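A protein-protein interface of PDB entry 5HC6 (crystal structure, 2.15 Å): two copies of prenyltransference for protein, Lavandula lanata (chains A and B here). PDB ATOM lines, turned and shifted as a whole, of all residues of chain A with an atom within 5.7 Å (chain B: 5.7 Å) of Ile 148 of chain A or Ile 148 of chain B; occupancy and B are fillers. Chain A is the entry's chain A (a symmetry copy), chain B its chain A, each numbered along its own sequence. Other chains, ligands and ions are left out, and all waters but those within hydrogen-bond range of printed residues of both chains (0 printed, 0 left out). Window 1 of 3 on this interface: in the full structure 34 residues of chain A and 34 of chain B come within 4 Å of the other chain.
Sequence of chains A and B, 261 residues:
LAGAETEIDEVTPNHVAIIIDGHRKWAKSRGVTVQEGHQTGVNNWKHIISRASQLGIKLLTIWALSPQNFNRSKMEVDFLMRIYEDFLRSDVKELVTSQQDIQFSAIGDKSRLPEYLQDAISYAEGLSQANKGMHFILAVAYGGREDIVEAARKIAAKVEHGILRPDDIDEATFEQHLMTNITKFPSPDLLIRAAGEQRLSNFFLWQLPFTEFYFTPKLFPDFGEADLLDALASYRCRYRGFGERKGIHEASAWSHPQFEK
Among the printed residues, merely in contact across the chains: Leu 205 of chain A with Leu 205 of chain B (3.3 Å), Ala 152 of chain A with Phe 174 of chain B (3.6 Å), Phe 174 of chain A with Ala 152 of chain B (3.6 Å), Trp 206 of chain A with Val 149 of chain B (3.8 Å), Val 149 of chain A with Trp 206 of chain B (3.8 Å), Trp 206 of chain A with Ile 148 of chain B (3.9 Å), Ile 148 of chain A with Trp 206 of chain B (3.9 Å) and Ile 148 of chain A with Ile 148 of chain B (3.98 Å).
Printed residues of chain A that touch a printed residue of chain B: Arg 145, Ile 148, Val 149, Ala 152, Phe 174, Leu 205 and Trp 206. Hydrophobic or aromatic side chains of chain A within 4 Å of the printed part of chain B: Ile 148, Val 149, Ala 152, Phe 174, Leu 205 and Trp 206. Hydrophobic or aromatic side chains of chain B that line the printed part of chain A: Ile 148, Val 149, Ala 152, Phe 174, Leu 205 and Trp 206. Among the printed residues, 10 pairs touch across the chains.
O of Trp 206 of chain A lies within hydrogen-bond range of NE of Arg 145 of chain B (2.7 Å). NE of Arg 145 of chain A is in hydrogen-bond range of O of Trp 206 of chain B, 2.7 Å away.
Of the printed residues of chain B, Ile 148 of chain A touches Ile 148 and Trp 206. Of the printed residues of chain A, Arg 145 of chain B touches Trp 206. Of the printed residues of chain A, Ile 148 of chain B touches Ile 148 (3.98 Å) and Trp 206 (3.9 Å). Printed residues of chain A within 4 Å of Trp 206 of chain B: Arg 145, Ile 148 and Val 149. The nearest printed residue of chain B that does not touch Ile 148 of chain A is Phe 174 of chain B (4.1 Å). The nearest printed residue of chain A that does not touch Ile 148 of chain B is Phe 174 of chain A (4.1 Å).
Ile 148 of chain A touches Trp 206 of chain B, and with the chains exchanged Trp 206 of chain A touches Ile 148 of chain B. Val 149 of chain A touches Trp 206 of chain B, and with the chains exchanged Trp 206 of chain A touches Val 149 of chain B. Ala 152 of chain A touches Phe 174 of chain B, and with the chains exchanged Phe 174 of chain A touches Ala 152 of chain B. Leu 205 of chain A touches its own counterpart, Leu 205 of chain B. 15 positions are printed for both chains.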
ATOM      1  N   GLY A 143      -6.078  26.695  23.740  1.00  0.00           N
ATOM      2  CA  GLY A 143      -6.454  25.463  24.361  1.00  0.00           C
ATOM      3  C   GLY A 143      -7.213  24.526  23.433  1.00  0.00           C
ATOM      4  O   GLY A 143      -8.047  24.949  22.591  1.00  0.00           O
ATOM      5  N   GLY A 144      -6.941  23.247  23.582  1.00  0.00           N
ATOM      6  CA  GLY A 144      -7.445  22.234  22.653  1.00  0.00           C
ATOM      7  C   GLY A 144      -8.934  22.087  22.715  1.00  0.00           C
ATOM      8  O   GLY A 144      -9.594  21.956  21.662  1.00  0.00           O
ATOM      9  N   ARG A 145      -9.489  22.101  23.943  1.00  0.00           N
ATOM     10  CA  ARG A 145     -10.951  22.007  24.109  1.00  0.00           C
ATOM     11  C   ARG A 145     -11.625  23.184  23.478  1.00  0.00           C
ATOM     12  O   ARG A 145     -12.628  23.036  22.803  1.00  0.00           O
ATOM     13  CB  ARG A 145     -11.343  21.999  25.585  1.00  0.00           C
ATOM     14  CG  ARG A 145     -11.034  20.723  26.340  1.00  0.00           C
ATOM     15  CD  ARG A 145     -12.135  19.761  26.126  1.00  0.00           C
ATOM     16  NE  ARG A 145     -12.006  18.464  26.820  1.00  0.00           N
ATOM     17  CZ  ARG A 145     -12.535  18.157  28.002  1.00  0.00           C
ATOM     18  NH1 ARG A 145     -13.154  19.091  28.704  1.00  0.00           N
ATOM     19  NH2 ARG A 145     -12.434  16.911  28.473  1.00  0.00           N
ATOM     20  N   GLU A 146     -11.118  24.378  23.775  1.00  0.00           N
ATOM     21  CA  GLU A 146     -11.661  25.633  23.214  1.00  0.00           C
ATOM     22  C   GLU A 146     -11.620  25.662  21.682  1.00  0.00           C
ATOM     23  O   GLU A 146     -12.570  26.121  21.020  1.00  0.00           O
ATOM     24  CB  GLU A 146     -10.841  26.822  23.682  1.00  0.00           C
ATOM     25  CG  GLU A 146     -11.067  27.187  25.133  1.00  0.00           C
ATOM     26  CD  GLU A 146     -10.348  26.309  26.177  1.00  0.00           C
ATOM     27  OE1 GLU A 146      -9.556  25.368  25.881  1.00  0.00           O
ATOM     28  OE2 GLU A 146     -10.574  26.585  27.346  1.00  0.00           O
ATOM     29  N   ASP A 147     -10.520  25.190  21.105  1.00  0.00           N
ATOM     30  CA  ASP A 147     -10.411  25.058  19.631  1.00  0.00           C
ATOM     31  C   ASP A 147     -11.514  24.175  19.098  1.00  0.00           C
ATOM     32  O   ASP A 147     -12.189  24.534  18.167  1.00  0.00           O
ATOM     33  CB  ASP A 147      -9.075  24.449  19.304  1.00  0.00           C
ATOM     34  CG  ASP A 147      -8.671  24.610  17.869  1.00  0.00           C
ATOM     35  OD1 ASP A 147      -9.399  25.248  17.047  1.00  0.00           O
ATOM     36  OD2 ASP A 147      -7.599  24.035  17.560  1.00  0.00           O
ATOM     37  N   ILE A 148     -11.710  22.991  19.667  1.00  0.00           N
ATOM     38  CA  ILE A 148     -12.745  22.129  19.194  1.00  0.00           C
ATOM     39  C   ILE A 148     -14.142  22.800  19.357  1.00  0.00           C
ATOM     40  O   ILE A 148     -14.994  22.675  18.471  1.00  0.00           O
ATOM     41  CB  ILE A 148     -12.724  20.842  19.945  1.00  0.00           C
ATOM     42  CG1 ILE A 148     -11.498  20.005  19.547  1.00  0.00           C
ATOM     43  CG2 ILE A 148     -13.940  20.015  19.644  1.00  0.00           C
ATOM     44  CD1 ILE A 148     -11.234  18.856  20.468  1.00  0.00           C
ATOM     45  N   VAL A 149     -14.386  23.474  20.500  1.00  0.00           N
ATOM     46  CA  VAL A 149     -15.672  24.081  20.755  1.00  0.00           C
ATOM     47  C   VAL A 149     -15.925  25.178  19.716  1.00  0.00           C
ATOM     48  O   VAL A 149     -17.002  25.268  19.112  1.00  0.00           O
ATOM     49  CB  VAL A 149     -15.799  24.633  22.223  1.00  0.00           C
ATOM     50  CG1 VAL A 149     -17.070  25.489  22.389  1.00  0.00           C
ATOM     51  CG2 VAL A 149     -15.859  23.479  23.205  1.00  0.00           C
ATOM     52  N   GLU A 150     -14.924  26.005  19.509  1.00  0.00           N
ATOM     53  CA  GLU A 150     -15.054  27.073  18.509  1.00  0.00           C
ATOM     54  C   GLU A 150     -15.243  26.490  17.104  1.00  0.00           C
ATOM     55  O   GLU A 150     -16.039  26.988  16.332  1.00  0.00           O
ATOM     56  CB  GLU A 150     -13.856  27.974  18.583  1.00  0.00           C
ATOM     57  CG  GLU A 150     -13.796  29.031  17.493  1.00  0.00           C
ATOM     58  CD  GLU A 150     -14.905  30.078  17.610  1.00  0.00           C
ATOM     59  OE1 GLU A 150     -15.484  30.218  18.695  1.00  0.00           O
ATOM     60  OE2 GLU A 150     -15.173  30.757  16.600  1.00  0.00           O
ATOM     61  N   ALA A 151     -14.542  25.426  16.749  1.00  0.00           N
ATOM     62  CA  ALA A 151     -14.817  24.823  15.450  1.00  0.00           C
ATOM     63  C   ALA A 151     -16.283  24.419  15.354  1.00  0.00           C
ATOM     64  O   ALA A 151     -16.929  24.641  14.340  1.00  0.00           O
ATOM     65  CB  ALA A 151     -13.917  23.623  15.169  1.00  0.00           C
ATOM     66  N   ALA A 152     -16.809  23.829  16.420  1.00  0.00           N
ATOM     67  CA  ALA A 152     -18.159  23.311  16.372  1.00  0.00           C
ATOM     68  C   ALA A 152     -19.181  24.469  16.293  1.00  0.00           C
ATOM     69  O   ALA A 152     -20.232  24.322  15.720  1.00  0.00           O
ATOM     70  CB  ALA A 152     -18.430  22.422  17.561  1.00  0.00           C
ATOM     71  N   ARG A 153     -18.828  25.604  16.873  1.00  0.00           N
ATOM     72  CA  ARG A 153     -19.660  26.772  16.885  1.00  0.00           C
ATOM     73  C   ARG A 153     -19.767  27.325  15.488  1.00  0.00           C
ATOM     74  O   ARG A 153     -20.864  27.666  15.019  1.00  0.00           O
ATOM     75  CB  ARG A 153     -19.020  27.835  17.745  1.00  0.00           C
ATOM     76  CG  ARG A 153     -19.344  27.771  19.198  1.00  0.00           C
ATOM     77  CD  ARG A 153     -19.041  29.112  19.851  1.00  0.00           C
ATOM     78  NE  ARG A 153     -19.839  29.218  21.058  1.00  0.00           N
ATOM     79  CZ  ARG A 153     -19.379  29.247  22.305  1.00  0.00           C
ATOM     80  NH1 ARG A 153     -18.079  29.224  22.576  1.00  0.00           N
ATOM     81  NH2 ARG A 153     -20.251  29.322  23.304  1.00  0.00           N
ATOM     82  N   PHE A 174     -14.493  19.279   9.760  1.00  0.00           N
ATOM     83  CA  PHE A 174     -14.135  19.703  11.121  1.00  0.00           C
ATOM     84  C   PHE A 174     -12.749  20.316  11.214  1.00  0.00           C
ATOM     85  O   PHE A 174     -12.526  21.320  11.869  1.00  0.00           O
ATOM     86  CB  PHE A 174     -14.272  18.547  12.138  1.00  0.00           C
ATOM     87  CG  PHE A 174     -14.596  19.036  13.530  1.00  0.00           C
ATOM     88  CD1 PHE A 174     -15.900  19.298  13.891  1.00  0.00           C
ATOM     89  CD2 PHE A 174     -13.581  19.284  14.443  1.00  0.00           C
ATOM     90  CE1 PHE A 174     -16.198  19.774  15.156  1.00  0.00           C
ATOM     91  CE2 PHE A 174     -13.863  19.777  15.699  1.00  0.00           C
ATOM     92  CZ  PHE A 174     -15.172  20.035  16.053  1.00  0.00           C
ATOM     93  N   LEU A 178     -10.810  24.484  12.662  1.00  0.00           N
ATOM     94  CA  LEU A 178      -9.924  24.574  13.791  1.00  0.00           C
ATOM     95  C   LEU A 178      -8.929  25.704  13.608  1.00  0.00           C
ATOM     96  O   LEU A 178      -8.583  26.077  12.493  1.00  0.00           O
ATOM     97  CB  LEU A 178      -9.179  23.252  13.886  1.00  0.00           C
ATOM     98  CG  LEU A 178      -9.620  22.127  14.803  1.00  0.00           C
ATOM     99  CD1 LEU A 178     -10.892  22.274  15.605  1.00  0.00           C
ATOM    100  CD2 LEU A 178      -9.487  20.781  14.148  1.00  0.00           C
ATOM    101  N   LEU A 205      -5.799  18.661  21.108  1.00  0.00           N
ATOM    102  CA  LEU A 205      -6.480  17.387  21.355  1.00  0.00           C
ATOM    103  C   LEU A 205      -6.878  16.701  20.061  1.00  0.00           C
ATOM    104  O   LEU A 205      -6.433  15.599  19.745  1.00  0.00           O
ATOM    105  CB  LEU A 205      -7.699  17.716  22.194  1.00  0.00           C
ATOM    106  CG  LEU A 205      -7.617  17.718  23.733  1.00  0.00           C
ATOM    107  CD1 LEU A 205      -6.308  17.504  24.467  1.00  0.00           C
ATOM    108  CD2 LEU A 205      -8.472  18.807  24.312  1.00  0.00           C
ATOM    109  N   TRP A 206      -7.720  17.362  19.278  1.00  0.00           N
ATOM    110  CA  TRP A 206      -8.087  16.877  17.955  1.00  0.00           C
ATOM    111  C   TRP A 206      -6.821  16.525  17.096  1.00  0.00           C
ATOM    112  O   TRP A 206      -6.772  15.572  16.344  1.00  0.00           O
ATOM    113  CB  TRP A 206      -8.882  17.989  17.239  1.00  0.00           C
ATOM    114  CG  TRP A 206      -9.050  17.653  15.777  1.00  0.00           C
ATOM    115  CD1 TRP A 206      -8.157  17.888  14.779  1.00  0.00           C
ATOM    116  CD2 TRP A 206     -10.169  16.984  15.178  1.00  0.00           C
ATOM    117  NE1 TRP A 206      -8.643  17.390  13.600  1.00  0.00           N
ATOM    118  CE2 TRP A 206      -9.875  16.833  13.811  1.00  0.00           C
ATOM    119  CE3 TRP A 206     -11.396  16.489  15.671  1.00  0.00           C
ATOM    120  CZ2 TRP A 206     -10.761  16.211  12.924  1.00  0.00           C
ATOM    121  CZ3 TRP A 206     -12.274  15.877  14.798  1.00  0.00           C
ATOM    122  CH2 TRP A 206     -11.947  15.736  13.433  1.00  0.00           C
ATOM    123  N   GLY B 143     -13.224   5.379  18.146  1.00  0.00           N
ATOM    124  CA  GLY B 143     -12.173   6.301  17.847  1.00  0.00           C
ATOM    125  C   GLY B 143     -12.484   7.730  18.266  1.00  0.00           C
ATOM    126  O   GLY B 143     -13.638   8.221  18.165  1.00  0.00           O
ATOM    127  N   GLY B 144     -11.460   8.413  18.733  1.00  0.00           N
ATOM    128  CA  GLY B 144     -11.623   9.733  19.345  1.00  0.00           C
ATOM    129  C   GLY B 144     -12.072  10.770  18.364  1.00  0.00           C
ATOM    130  O   GLY B 144     -12.942  11.605  18.690  1.00  0.00           O
ATOM    131  N   ARG B 145     -11.487  10.743  17.149  1.00  0.00           N
ATOM    132  CA  ARG B 145     -11.890  11.695  16.098  1.00  0.00           C
ATOM    133  C   ARG B 145     -13.325  11.487  15.728  1.00  0.00           C
ATOM    134  O   ARG B 145     -14.069  12.439  15.574  1.00  0.00           O
ATOM    135  CB  ARG B 145     -11.063  11.502  14.828  1.00  0.00           C
ATOM    136  CG  ARG B 145      -9.627  11.976  14.902  1.00  0.00           C
ATOM    137  CD  ARG B 145      -9.584  13.424  14.614  1.00  0.00           C
ATOM    138  NE  ARG B 145      -8.244  14.046  14.617  1.00  0.00           N
ATOM    139  CZ  ARG B 145      -7.475  14.243  13.550  1.00  0.00           C
ATOM    140  NH1 ARG B 145      -7.851  13.766  12.375  1.00  0.00           N
ATOM    141  NH2 ARG B 145      -6.326  14.914  13.671  1.00  0.00           N
ATOM    142  N   GLU B 146     -13.694  10.230  15.497  1.00  0.00           N
ATOM    143  CA  GLU B 146     -15.081   9.863  15.141  1.00  0.00           C
ATOM    144  C   GLU B 146     -16.095  10.281  16.211  1.00  0.00           C
ATOM    145  O   GLU B 146     -17.199  10.766  15.898  1.00  0.00           O
ATOM    146  CB  GLU B 146     -15.211   8.356  15.001  1.00  0.00           C
ATOM    147  CG  GLU B 146     -14.574   7.802  13.744  1.00  0.00           C
ATOM    148  CD  GLU B 146     -13.040   7.644  13.770  1.00  0.00           C
ATOM    149  OE1 GLU B 146     -12.324   7.892  14.783  1.00  0.00           O
ATOM    150  OE2 GLU B 146     -12.534   7.239  12.734  1.00  0.00           O
ATOM    151  N   ASP B 147     -15.743  10.085  17.477  1.00  0.00           N
ATOM    152  CA  ASP B 147     -16.590  10.557  18.602  1.00  0.00           C
ATOM    153  C   ASP B 147     -16.810  12.048  18.506  1.00  0.00           C
ATOM    154  O   ASP B 147     -17.919  12.509  18.591  1.00  0.00           O
ATOM    155  CB  ASP B 147     -15.893  10.231  19.893  1.00  0.00           C
ATOM    156  CG  ASP B 147     -16.786  10.295  21.096  1.00  0.00           C
ATOM    157  OD1 ASP B 147     -18.023  10.560  20.986  1.00  0.00           O
ATOM    158  OD2 ASP B 147     -16.201  10.108  22.191  1.00  0.00           O
ATOM    159  N   ILE B 148     -15.753  12.836  18.346  1.00  0.00           N
ATOM    160  CA  ILE B 148     -15.920  14.250  18.249  1.00  0.00           C
ATOM    161  C   ILE B 148     -16.788  14.621  17.010  1.00  0.00           C
ATOM    162  O   ILE B 148     -17.628  15.525  17.093  1.00  0.00           O
ATOM    163  CB  ILE B 148     -14.591  14.917  18.139  1.00  0.00           C
ATOM    164  CG1 ILE B 148     -13.838  14.844  19.476  1.00  0.00           C
ATOM    165  CG2 ILE B 148     -14.737  16.370  17.792  1.00  0.00           C
ATOM    166  CD1 ILE B 148     -12.390  15.206  19.368  1.00  0.00           C
ATOM    167  N   VAL B 149     -16.560  13.955  15.859  1.00  0.00           N
ATOM    168  CA  VAL B 149     -17.285  14.272  14.650  1.00  0.00           C
ATOM    169  C   VAL B 149     -18.772  13.975  14.862  1.00  0.00           C
ATOM    170  O   VAL B 149     -19.651  14.785  14.539  1.00  0.00           O
ATOM    171  CB  VAL B 149     -16.718  13.518  13.391  1.00  0.00           C
ATOM    172  CG1 VAL B 149     -17.654  13.677  12.177  1.00  0.00           C
ATOM    173  CG2 VAL B 149     -15.354  14.072  13.028  1.00  0.00           C
ATOM    174  N   GLU B 150     -19.046  12.814  15.415  1.00  0.00           N
ATOM    175  CA  GLU B 150     -20.441  12.448  15.691  1.00  0.00           C
ATOM    176  C   GLU B 150     -21.071  13.407  16.707  1.00  0.00           C
ATOM    177  O   GLU B 150     -22.211  13.799  16.560  1.00  0.00           O
ATOM    178  CB  GLU B 150     -20.500  11.022  16.158  1.00  0.00           C
ATOM    179  CG  GLU B 150     -21.873  10.570  16.624  1.00  0.00           C
ATOM    180  CD  GLU B 150     -22.901  10.505  15.493  1.00  0.00           C
ATOM    181  OE1 GLU B 150     -22.500  10.447  14.323  1.00  0.00           O
ATOM    182  OE2 GLU B 150     -24.108  10.504  15.803  1.00  0.00           O
ATOM    183  N   ALA B 151     -20.349  13.817  17.737  1.00  0.00           N
ATOM    184  CA  ALA B 151     -20.930  14.813  18.631  1.00  0.00           C
ATOM    185  C   ALA B 151     -21.309  16.066  17.850  1.00  0.00           C
ATOM    186  O   ALA B 151     -22.374  16.631  18.052  1.00  0.00           O
ATOM    187  CB  ALA B 151     -19.995  15.169  19.783  1.00  0.00           C
ATOM    188  N   ALA B 152     -20.434  16.495  16.951  1.00  0.00           N
ATOM    189  CA  ALA B 152     -20.662  17.739  16.249  1.00  0.00           C
ATOM    190  C   ALA B 152     -21.857  17.600  15.275  1.00  0.00           C
ATOM    191  O   ALA B 152     -22.553  18.551  15.019  1.00  0.00           O
ATOM    192  CB  ALA B 152     -19.415  18.178  15.524  1.00  0.00           C
ATOM    193  N   ARG B 153     -22.062  16.397  14.766  1.00  0.00           N
ATOM    194  CA  ARG B 153     -23.127  16.101  13.853  1.00  0.00           C
ATOM    195  C   ARG B 153     -24.446  16.204  14.573  1.00  0.00           C
ATOM    196  O   ARG B 153     -25.405  16.808  14.067  1.00  0.00           O
ATOM    197  CB  ARG B 153     -22.989  14.680  13.363  1.00  0.00           C
ATOM    198  CG  ARG B 153     -22.115  14.492  12.171  1.00  0.00           C
ATOM    199  CD  ARG B 153     -22.422  13.153  11.515  1.00  0.00           C
ATOM    200  NE  ARG B 153     -22.005  13.222  10.128  1.00  0.00           N
ATOM    201  CZ  ARG B 153     -21.020  12.528   9.567  1.00  0.00           C
ATOM    202  NH1 ARG B 153     -20.316  11.630  10.247  1.00  0.00           N
ATOM    203  NH2 ARG B 153     -20.749  12.730   8.283  1.00  0.00           N
ATOM    204  N   PHE B 174     -21.014  20.247  24.434  1.00  0.00           N
ATOM    205  CA  PHE B 174     -20.245  19.305  23.608  1.00  0.00           C
ATOM    206  C   PHE B 174     -20.033  17.957  24.274  1.00  0.00           C
ATOM    207  O   PHE B 174     -20.156  16.907  23.667  1.00  0.00           O
ATOM    208  CB  PHE B 174     -18.888  19.899  23.171  1.00  0.00           C
ATOM    209  CG  PHE B 174     -18.408  19.339  21.852  1.00  0.00           C
ATOM    210  CD1 PHE B 174     -18.848  19.879  20.663  1.00  0.00           C
ATOM    211  CD2 PHE B 174     -17.566  18.237  21.822  1.00  0.00           C
ATOM    212  CE1 PHE B 174     -18.433  19.349  19.454  1.00  0.00           C
ATOM    213  CE2 PHE B 174     -17.161  17.688  20.623  1.00  0.00           C
ATOM    214  CZ  PHE B 174     -17.606  18.236  19.437  1.00  0.00           C
ATOM    215  N   LEU B 178     -20.984  13.335  23.294  1.00  0.00           N
ATOM    216  CA  LEU B 178     -19.949  12.361  23.079  1.00  0.00           C
ATOM    217  C   LEU B 178     -20.403  10.982  23.518  1.00  0.00           C
ATOM    218  O   LEU B 178     -21.243  10.837  24.399  1.00  0.00           O
ATOM    219  CB  LEU B 178     -18.748  12.788  23.906  1.00  0.00           C
ATOM    220  CG  LEU B 178     -17.594  13.586  23.328  1.00  0.00           C
ATOM    221  CD1 LEU B 178     -17.658  14.052  21.893  1.00  0.00           C
ATOM    222  CD2 LEU B 178     -17.114  14.650  24.275  1.00  0.00           C
ATOM    223  N   LEU B 205      -9.712  11.670  22.578  1.00  0.00           N
ATOM    224  CA  LEU B 205      -9.000  12.930  22.347  1.00  0.00           C
ATOM    225  C   LEU B 205      -9.573  14.062  23.180  1.00  0.00           C
ATOM    226  O   LEU B 205      -8.902  14.650  24.026  1.00  0.00           O
ATOM    227  CB  LEU B 205      -9.134  13.223  20.865  1.00  0.00           C
ATOM    228  CG  LEU B 205      -8.086  12.701  19.862  1.00  0.00           C
ATOM    229  CD1 LEU B 205      -6.951  11.791  20.289  1.00  0.00           C
ATOM    230  CD2 LEU B 205      -8.736  12.304  18.569  1.00  0.00           C
ATOM    231  N   TRP B 206     -10.843  14.372  22.960  1.00  0.00           N
ATOM    232  CA  TRP B 206     -11.550  15.352  23.773  1.00  0.00           C
ATOM    233  C   TRP B 206     -11.397  15.051  25.306  1.00  0.00           C
ATOM    234  O   TRP B 206     -11.264  15.920  26.144  1.00  0.00           O
ATOM    235  CB  TRP B 206     -13.047  15.293  23.402  1.00  0.00           C
ATOM    236  CG  TRP B 206     -13.863  16.082  24.396  1.00  0.00           C
ATOM    237  CD1 TRP B 206     -14.324  15.648  25.599  1.00  0.00           C
ATOM    238  CD2 TRP B 206     -14.270  17.452  24.270  1.00  0.00           C
ATOM    239  NE1 TRP B 206     -14.974  16.669  26.239  1.00  0.00           N
ATOM    240  CE2 TRP B 206     -14.962  17.786  25.449  1.00  0.00           C
ATOM    241  CE3 TRP B 206     -14.108  18.437  23.272  1.00  0.00           C
ATOM    242  CZ2 TRP B 206     -15.496  19.061  25.661  1.00  0.00           C
ATOM    243  CZ3 TRP B 206     -14.638  19.696  23.477  1.00  0.00           C
ATOM    244  CH2 TRP B 206     -15.321  20.001  24.673  1.00  0.00           C
